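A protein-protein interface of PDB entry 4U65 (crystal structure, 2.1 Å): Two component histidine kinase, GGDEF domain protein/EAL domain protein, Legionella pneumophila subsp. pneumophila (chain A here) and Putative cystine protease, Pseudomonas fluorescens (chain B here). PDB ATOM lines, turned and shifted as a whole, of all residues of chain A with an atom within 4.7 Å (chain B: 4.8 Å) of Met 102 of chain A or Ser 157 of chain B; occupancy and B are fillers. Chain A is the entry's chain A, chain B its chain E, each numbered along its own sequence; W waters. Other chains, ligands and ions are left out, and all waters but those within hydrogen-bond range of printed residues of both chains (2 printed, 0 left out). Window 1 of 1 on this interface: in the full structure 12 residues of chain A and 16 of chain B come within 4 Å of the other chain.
OE1 of Gln 107 of chain A lies within hydrogen-bond range of NE of Arg 107 of chain B (2.7 Å). OH of Tyr 156 of chain B lies within hydrogen-bond range of O of Leu 100 of chain A (2.5 Å). The side-chain hydroxyl of Tyr 126 of chain B is in hydrogen-bond range of the backbone carbonyl oxygen of Trp 105 of chain A, 2.6 Å away.
The side-chain hydroxyl (OG) of Ser 33 of chain A sits at hydrogen-bond distance from the backbone NH (N) of Met 102 of chain A, 3.0 Å away. The side-chain amide oxygen of Asn 159 of chain B lies close to the guanidinium group of Arg 107 of chain B, at 3.4 Å.
Among the printed residues, merely in contact across the chains: Ser 33 of chain A with Tyr 156 of chain B (3.5 Å), Leu 100 of chain A with Arg 107 of chain B (3.8 Å), Leu 100 of chain A with Ser 157 of chain B (3.9 Å), Met 102 of chain A with Tyr 126 of chain B (3.4 Å), Met 102 of chain A with Ser 157 of chain B (3.6 Å), Trp 105 of chain A with Thr 109 of chain B (3.97 Å) and Gln 107 of chain A with Tyr 126 of chain B (3.5 Å).
Printed residues of chain B within 4 Å of Ser 33 of chain A: Tyr 156. Met 102 of chain A touches two residues of chain B. Gly 104 of chain A touches none of the printed residues of chain B. Of the printed residues of chain B, Trp 105 of chain A touches Thr 109 (3.97 Å) and Tyr 126 (2.6 Å). Of the printed residues of chain A, Tyr 126 of chain B touches Met 102, Trp 105 and Gln 107. Of the printed residues of chain A, Tyr 156 of chain B touches Ser 33 and Leu 100. Phe 158 of chain B touches none of the printed residues of chain A. The nearest printed residue of chain A that does not touch Ser 157 of chain B is Gly 104 of chain A (4.9 Å). The nearest printed residue of chain A that does not touch Arg 107 of chain B is Met 102 of chain A (6.2 Å).
Of the 9 printed residues of chain B, 5 touch a printed residue of chain A. Printed residues of chain B that touch a printed residue of chain A: Arg 107, Thr 109, Tyr 126, Tyr 156 and Ser 157. Of the 11 printed residues of chain A, 5 touch a printed residue of chain B. Hydrophobic or aromatic side chains of chain A within 4 Å of the printed part of chain B: Leu 100, Met 102 and Trp 105. Among the printed residues, 10 pairs touch across the chains.
Water W2 lies within hydrogen-bond range of O of Ser 157 of chain B (2.8 Å) and N of Leu 100 of chain A (2.9 Å). Water W1 lies within hydrogen-bond range of OG of Ser 157 of chain B (2.8 Å) and O of Gly 104 of chain A (2.9 Å).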
ATOM      1  N   SER A  33      11.710 -24.754  34.526  1.00  0.00           N
ATOM      2  CA  SER A  33      11.258 -26.067  34.093  1.00  0.00           C
ATOM      3  C   SER A  33      12.209 -27.175  34.528  1.00  0.00           C
ATOM      4  O   SER A  33      11.837 -28.352  34.476  1.00  0.00           O
ATOM      5  CB  SER A  33      11.073 -26.087  32.574  1.00  0.00           C
ATOM      6  OG  SER A  33      10.029 -25.207  32.193  1.00  0.00           O
ATOM      7  N   ASN A  38      10.347 -25.375  39.973  1.00  0.00           N
ATOM      8  CA  ASN A  38       9.136 -24.602  40.212  1.00  0.00           C
ATOM      9  C   ASN A  38       8.328 -25.116  41.397  1.00  0.00           C
ATOM     10  O   ASN A  38       7.372 -24.447  41.803  1.00  0.00           O
ATOM     11  CB  ASN A  38       8.264 -24.603  38.954  1.00  0.00           C
ATOM     12  CG  ASN A  38       7.823 -26.001  38.549  1.00  0.00           C
ATOM     13  OD1 ASN A  38       6.803 -26.500  39.019  1.00  0.00           O
ATOM     14  ND2 ASN A  38       8.597 -26.639  37.677  1.00  0.00           N
ATOM     15  N   LEU A 100       5.460 -21.182  29.251  1.00  0.00           N
ATOM     16  CA  LEU A 100       5.051 -22.312  30.079  1.00  0.00           C
ATOM     17  C   LEU A 100       6.147 -22.775  31.036  1.00  0.00           C
ATOM     18  O   LEU A 100       7.343 -22.697  30.739  1.00  0.00           O
ATOM     19  CB  LEU A 100       4.637 -23.491  29.198  1.00  0.00           C
ATOM     20  CG  LEU A 100       3.462 -23.272  28.246  1.00  0.00           C
ATOM     21  CD1 LEU A 100       3.219 -24.520  27.406  1.00  0.00           C
ATOM     22  CD2 LEU A 100       2.212 -22.887  29.021  1.00  0.00           C
ATOM     23  N   ILE A 101       5.721 -23.243  32.208  1.00  0.00           N
ATOM     24  CA  ILE A 101       6.590 -23.931  33.157  1.00  0.00           C
ATOM     25  C   ILE A 101       6.259 -25.420  33.095  1.00  0.00           C
ATOM     26  O   ILE A 101       5.102 -25.815  33.295  1.00  0.00           O
ATOM     27  CB  ILE A 101       6.422 -23.378  34.580  1.00  0.00           C
ATOM     28  CG1 ILE A 101       6.711 -21.874  34.597  1.00  0.00           C
ATOM     29  CG2 ILE A 101       7.352 -24.089  35.536  1.00  0.00           C
ATOM     30  CD1 ILE A 101       6.510 -21.229  35.948  1.00  0.00           C
ATOM     31  N   MET A 102       7.264 -26.244  32.803  1.00  0.00           N
ATOM     32  CA  MET A 102       7.062 -27.652  32.483  1.00  0.00           C
ATOM     33  C   MET A 102       7.826 -28.558  33.441  1.00  0.00           C
ATOM     34  O   MET A 102       8.931 -28.223  33.881  1.00  0.00           O
ATOM     35  CB  MET A 102       7.488 -27.953  31.041  1.00  0.00           C
ATOM     36  CG  MET A 102       6.764 -27.121  29.989  1.00  0.00           C
ATOM     37  SD  MET A 102       5.004 -27.501  29.878  1.00  0.00           S
ATOM     38  CE  MET A 102       5.061 -29.221  29.372  1.00  0.00           C
ATOM     39  N   ASP A 103       7.229 -29.703  33.770  1.00  0.00           N
ATOM     40  CA  ASP A 103       7.933 -30.820  34.402  1.00  0.00           C
ATOM     41  C   ASP A 103       7.987 -31.950  33.377  1.00  0.00           C
ATOM     42  O   ASP A 103       7.138 -32.841  33.372  1.00  0.00           O
ATOM     43  CB  ASP A 103       7.248 -31.288  35.687  1.00  0.00           C
ATOM     44  CG  ASP A 103       7.328 -30.269  36.799  1.00  0.00           C
ATOM     45  OD1 ASP A 103       8.325 -29.515  36.854  1.00  0.00           O
ATOM     46  OD2 ASP A 103       6.394 -30.235  37.627  1.00  0.00           O
ATOM     47  N   GLY A 104       8.986 -31.908  32.499  1.00  0.00           N
ATOM     48  CA  GLY A 104       9.037 -32.887  31.433  1.00  0.00           C
ATOM     49  C   GLY A 104       7.859 -32.721  30.494  1.00  0.00           C
ATOM     50  O   GLY A 104       7.705 -31.673  29.860  1.00  0.00           O
ATOM     51  N   TRP A 105       7.011 -33.748  30.406  1.00  0.00           N
ATOM     52  CA  TRP A 105       5.814 -33.672  29.579  1.00  0.00           C
ATOM     53  C   TRP A 105       4.634 -33.036  30.295  1.00  0.00           C
ATOM     54  O   TRP A 105       3.666 -32.646  29.634  1.00  0.00           O
ATOM     55  CB  TRP A 105       5.365 -35.069  29.144  1.00  0.00           C
ATOM     56  CG  TRP A 105       6.327 -35.856  28.326  1.00  0.00           C
ATOM     57  CD1 TRP A 105       7.061 -36.926  28.744  1.00  0.00           C
ATOM     58  CD2 TRP A 105       6.634 -35.674  26.938  1.00  0.00           C
ATOM     59  NE1 TRP A 105       7.816 -37.416  27.708  1.00  0.00           N
ATOM     60  CE2 TRP A 105       7.570 -36.668  26.587  1.00  0.00           C
ATOM     61  CE3 TRP A 105       6.206 -34.773  25.958  1.00  0.00           C
ATOM     62  CZ2 TRP A 105       8.093 -36.780  25.301  1.00  0.00           C
ATOM     63  CZ3 TRP A 105       6.727 -34.885  24.681  1.00  0.00           C
ATOM     64  CH2 TRP A 105       7.660 -35.880  24.365  1.00  0.00           C
ATOM     65  N   MET A 106       4.684 -32.930  31.620  1.00  0.00           N
ATOM     66  CA  MET A 106       3.564 -32.424  32.402  1.00  0.00           C
ATOM     67  C   MET A 106       3.662 -30.911  32.532  1.00  0.00           C
ATOM     68  O   MET A 106       4.728 -30.381  32.862  1.00  0.00           O
ATOM     69  CB  MET A 106       3.555 -33.070  33.788  1.00  0.00           C
ATOM     70  CG  MET A 106       3.528 -34.590  33.756  1.00  0.00           C
ATOM     71  SD  MET A 106       2.071 -35.261  32.938  1.00  0.00           S
ATOM     72  CE  MET A 106       0.841 -34.979  34.208  1.00  0.00           C
ATOM     73  N   GLN A 107       2.548 -30.223  32.306  1.00  0.00           N
ATOM     74  CA  GLN A 107       2.518 -28.780  32.496  1.00  0.00           C
ATOM     75  C   GLN A 107       2.491 -28.461  33.983  1.00  0.00           C
ATOM     76  O   GLN A 107       1.759 -29.093  34.752  1.00  0.00           O
ATOM     77  CB  GLN A 107       1.313 -28.153  31.796  1.00  0.00           C
ATOM     78  CG  GLN A 107       1.309 -28.314  30.286  1.00  0.00           C
ATOM     79  CD  GLN A 107       0.118 -27.638  29.637  1.00  0.00           C
ATOM     80  OE1 GLN A 107       0.274 -26.660  28.908  1.00  0.00           O
ATOM     81  NE2 GLN A 107      -1.078 -28.152  29.901  1.00  0.00           N
ATOM     82  N   ALA A 108       3.323 -27.505  34.391  1.00  0.00           N
ATOM     83  CA  ALA A 108       3.438 -27.114  35.786  1.00  0.00           C
ATOM     84  C   ALA A 108       3.023 -25.672  36.039  1.00  0.00           C
ATOM     85  O   ALA A 108       3.047 -25.233  37.196  1.00  0.00           O
ATOM     86  CB  ALA A 108       4.874 -27.329  36.282  1.00  0.00           C
ATOM     87  N   ARG B 107       0.323 -27.955  21.996  1.00  0.00           N
ATOM     88  CA  ARG B 107       1.621 -27.349  22.252  1.00  0.00           C
ATOM     89  C   ARG B 107       2.638 -27.814  21.220  1.00  0.00           C
ATOM     90  O   ARG B 107       2.643 -28.980  20.814  1.00  0.00           O
ATOM     91  CB  ARG B 107       2.139 -27.682  23.660  1.00  0.00           C
ATOM     92  CG  ARG B 107       1.692 -26.722  24.753  1.00  0.00           C
ATOM     93  CD  ARG B 107       0.261 -26.969  25.182  1.00  0.00           C
ATOM     94  NE  ARG B 107      -0.115 -26.102  26.294  1.00  0.00           N
ATOM     95  CZ  ARG B 107      -0.718 -24.926  26.152  1.00  0.00           C
ATOM     96  NH1 ARG B 107      -1.017 -24.474  24.942  1.00  0.00           N
ATOM     97  NH2 ARG B 107      -1.023 -24.203  27.220  1.00  0.00           N
ATOM     98  N   ILE B 108       3.485 -26.884  20.791  1.00  0.00           N
ATOM     99  CA  ILE B 108       4.677 -27.209  20.016  1.00  0.00           C
ATOM    100  C   ILE B 108       5.781 -27.580  20.997  1.00  0.00           C
ATOM    101  O   ILE B 108       6.151 -26.775  21.859  1.00  0.00           O
ATOM    102  CB  ILE B 108       5.092 -26.026  19.129  1.00  0.00           C
ATOM    103  CG1 ILE B 108       4.012 -25.739  18.085  1.00  0.00           C
ATOM    104  CG2 ILE B 108       6.415 -26.302  18.458  1.00  0.00           C
ATOM    105  CD1 ILE B 108       3.796 -26.871  17.107  1.00  0.00           C
ATOM    106  N   THR B 109       6.317 -28.793  20.868  1.00  0.00           N
ATOM    107  CA  THR B 109       7.208 -29.361  21.877  1.00  0.00           C
ATOM    108  C   THR B 109       8.551 -29.726  21.260  1.00  0.00           C
ATOM    109  O   THR B 109       8.615 -30.557  20.347  1.00  0.00           O
ATOM    110  CB  THR B 109       6.572 -30.588  22.533  1.00  0.00           C
ATOM    111  OG1 THR B 109       5.303 -30.228  23.094  1.00  0.00           O
ATOM    112  CG2 THR B 109       7.474 -31.125  23.637  1.00  0.00           C
ATOM    113  N   TYR B 126      -3.149 -31.914  25.139  1.00  0.00           N
ATOM    114  CA  TYR B 126      -3.490 -31.992  26.557  1.00  0.00           C
ATOM    115  C   TYR B 126      -5.008 -31.955  26.690  1.00  0.00           C
ATOM    116  O   TYR B 126      -5.626 -30.901  26.506  1.00  0.00           O
ATOM    117  CB  TYR B 126      -2.848 -30.847  27.343  1.00  0.00           C
ATOM    118  CG  TYR B 126      -1.340 -30.920  27.419  1.00  0.00           C
ATOM    119  CD1 TYR B 126      -0.547 -30.517  26.350  1.00  0.00           C
ATOM    120  CD2 TYR B 126      -0.709 -31.397  28.561  1.00  0.00           C
ATOM    121  CE1 TYR B 126       0.833 -30.588  26.419  1.00  0.00           C
ATOM    122  CE2 TYR B 126       0.668 -31.471  28.640  1.00  0.00           C
ATOM    123  CZ  TYR B 126       1.435 -31.065  27.567  1.00  0.00           C
ATOM    124  OH  TYR B 126       2.807 -31.139  27.647  1.00  0.00           O
ATOM    125  N   VAL B 155      12.119 -31.353  26.027  1.00  0.00           N
ATOM    126  CA  VAL B 155      13.044 -30.277  26.361  1.00  0.00           C
ATOM    127  C   VAL B 155      12.299 -29.009  26.763  1.00  0.00           C
ATOM    128  O   VAL B 155      12.533 -28.453  27.840  1.00  0.00           O
ATOM    129  CB  VAL B 155      14.018 -29.994  25.197  1.00  0.00           C
ATOM    130  CG1 VAL B 155      14.877 -28.793  25.513  1.00  0.00           C
ATOM    131  CG2 VAL B 155      14.882 -31.217  24.922  1.00  0.00           C
ATOM    132  N   TYR B 156      11.391 -28.538  25.909  1.00  0.00           N
ATOM    133  CA  TYR B 156      10.555 -27.394  26.245  1.00  0.00           C
ATOM    134  C   TYR B 156       9.336 -27.397  25.337  1.00  0.00           C
ATOM    135  O   TYR B 156       9.339 -28.004  24.263  1.00  0.00           O
ATOM    136  CB  TYR B 156      11.322 -26.071  26.128  1.00  0.00           C
ATOM    137  CG  TYR B 156      10.683 -24.937  26.899  1.00  0.00           C
ATOM    138  CD1 TYR B 156      10.287 -25.109  28.219  1.00  0.00           C
ATOM    139  CD2 TYR B 156      10.478 -23.694  26.310  1.00  0.00           C
ATOM    140  CE1 TYR B 156       9.700 -24.080  28.932  1.00  0.00           C
ATOM    141  CE2 TYR B 156       9.892 -22.656  27.016  1.00  0.00           C
ATOM    142  CZ  TYR B 156       9.505 -22.855  28.327  1.00  0.00           C
ATOM    143  OH  TYR B 156       8.922 -21.832  29.039  1.00  0.00           O
ATOM    144  N   SER B 157       8.291 -26.698  25.782  1.00  0.00           N
ATOM    145  CA  SER B 157       7.014 -26.665  25.086  1.00  0.00           C
ATOM    146  C   SER B 157       6.526 -25.229  24.970  1.00  0.00           C
ATOM    147  O   SER B 157       6.785 -24.396  25.843  1.00  0.00           O
ATOM    148  CB  SER B 157       5.965 -27.515  25.810  1.00  0.00           C
ATOM    149  OG  SER B 157       6.490 -28.790  26.138  1.00  0.00           O
ATOM    150  N   PHE B 158       5.812 -24.949  23.884  1.00  0.00           N
ATOM    151  CA  PHE B 158       5.315 -23.611  23.598  1.00  0.00           C
ATOM    152  C   PHE B 158       3.830 -23.650  23.280  1.00  0.00           C
ATOM    153  O   PHE B 158       3.350 -24.565  22.603  1.00  0.00           O
ATOM    154  CB  PHE B 158       6.056 -22.974  22.416  1.00  0.00           C
ATOM    155  CG  PHE B 158       7.489 -22.642  22.700  1.00  0.00           C
ATOM    156  CD1 PHE B 158       7.835 -21.413  23.240  1.00  0.00           C
ATOM    157  CD2 PHE B 158       8.494 -23.550  22.410  1.00  0.00           C
ATOM    158  CE1 PHE B 158       9.154 -21.096  23.495  1.00  0.00           C
ATOM    159  CE2 PHE B 158       9.817 -23.239  22.663  1.00  0.00           C
ATOM    160  CZ  PHE B 158      10.148 -22.010  23.206  1.00  0.00           C
ATOM    161  N   ASN B 159       3.113 -22.642  23.762  1.00  0.00           N
ATOM    162  CA  ASN B 159       1.753 -22.367  23.320  1.00  0.00           C
ATOM    163  C   ASN B 159       1.814 -21.412  22.133  1.00  0.00           C
ATOM    164  O   ASN B 159       2.398 -20.327  22.233  1.00  0.00           O
ATOM    165  CB  ASN B 159       0.922 -21.785  24.462  1.00  0.00           C
ATOM    166  CG  ASN B 159      -0.197 -20.897  23.970  1.00  0.00           C
ATOM    167  OD1 ASN B 159      -1.215 -21.375  23.467  1.00  0.00           O
ATOM    168  ND2 ASN B 159      -0.028 -19.593  24.144  1.00  0.00           N
HETATM  169  O   HOH W   1       8.442 -29.618  27.971  1.00  0.00           O
HETATM  170  O   HOH W   2       6.333 -21.775  26.603  1.00  0.00           O
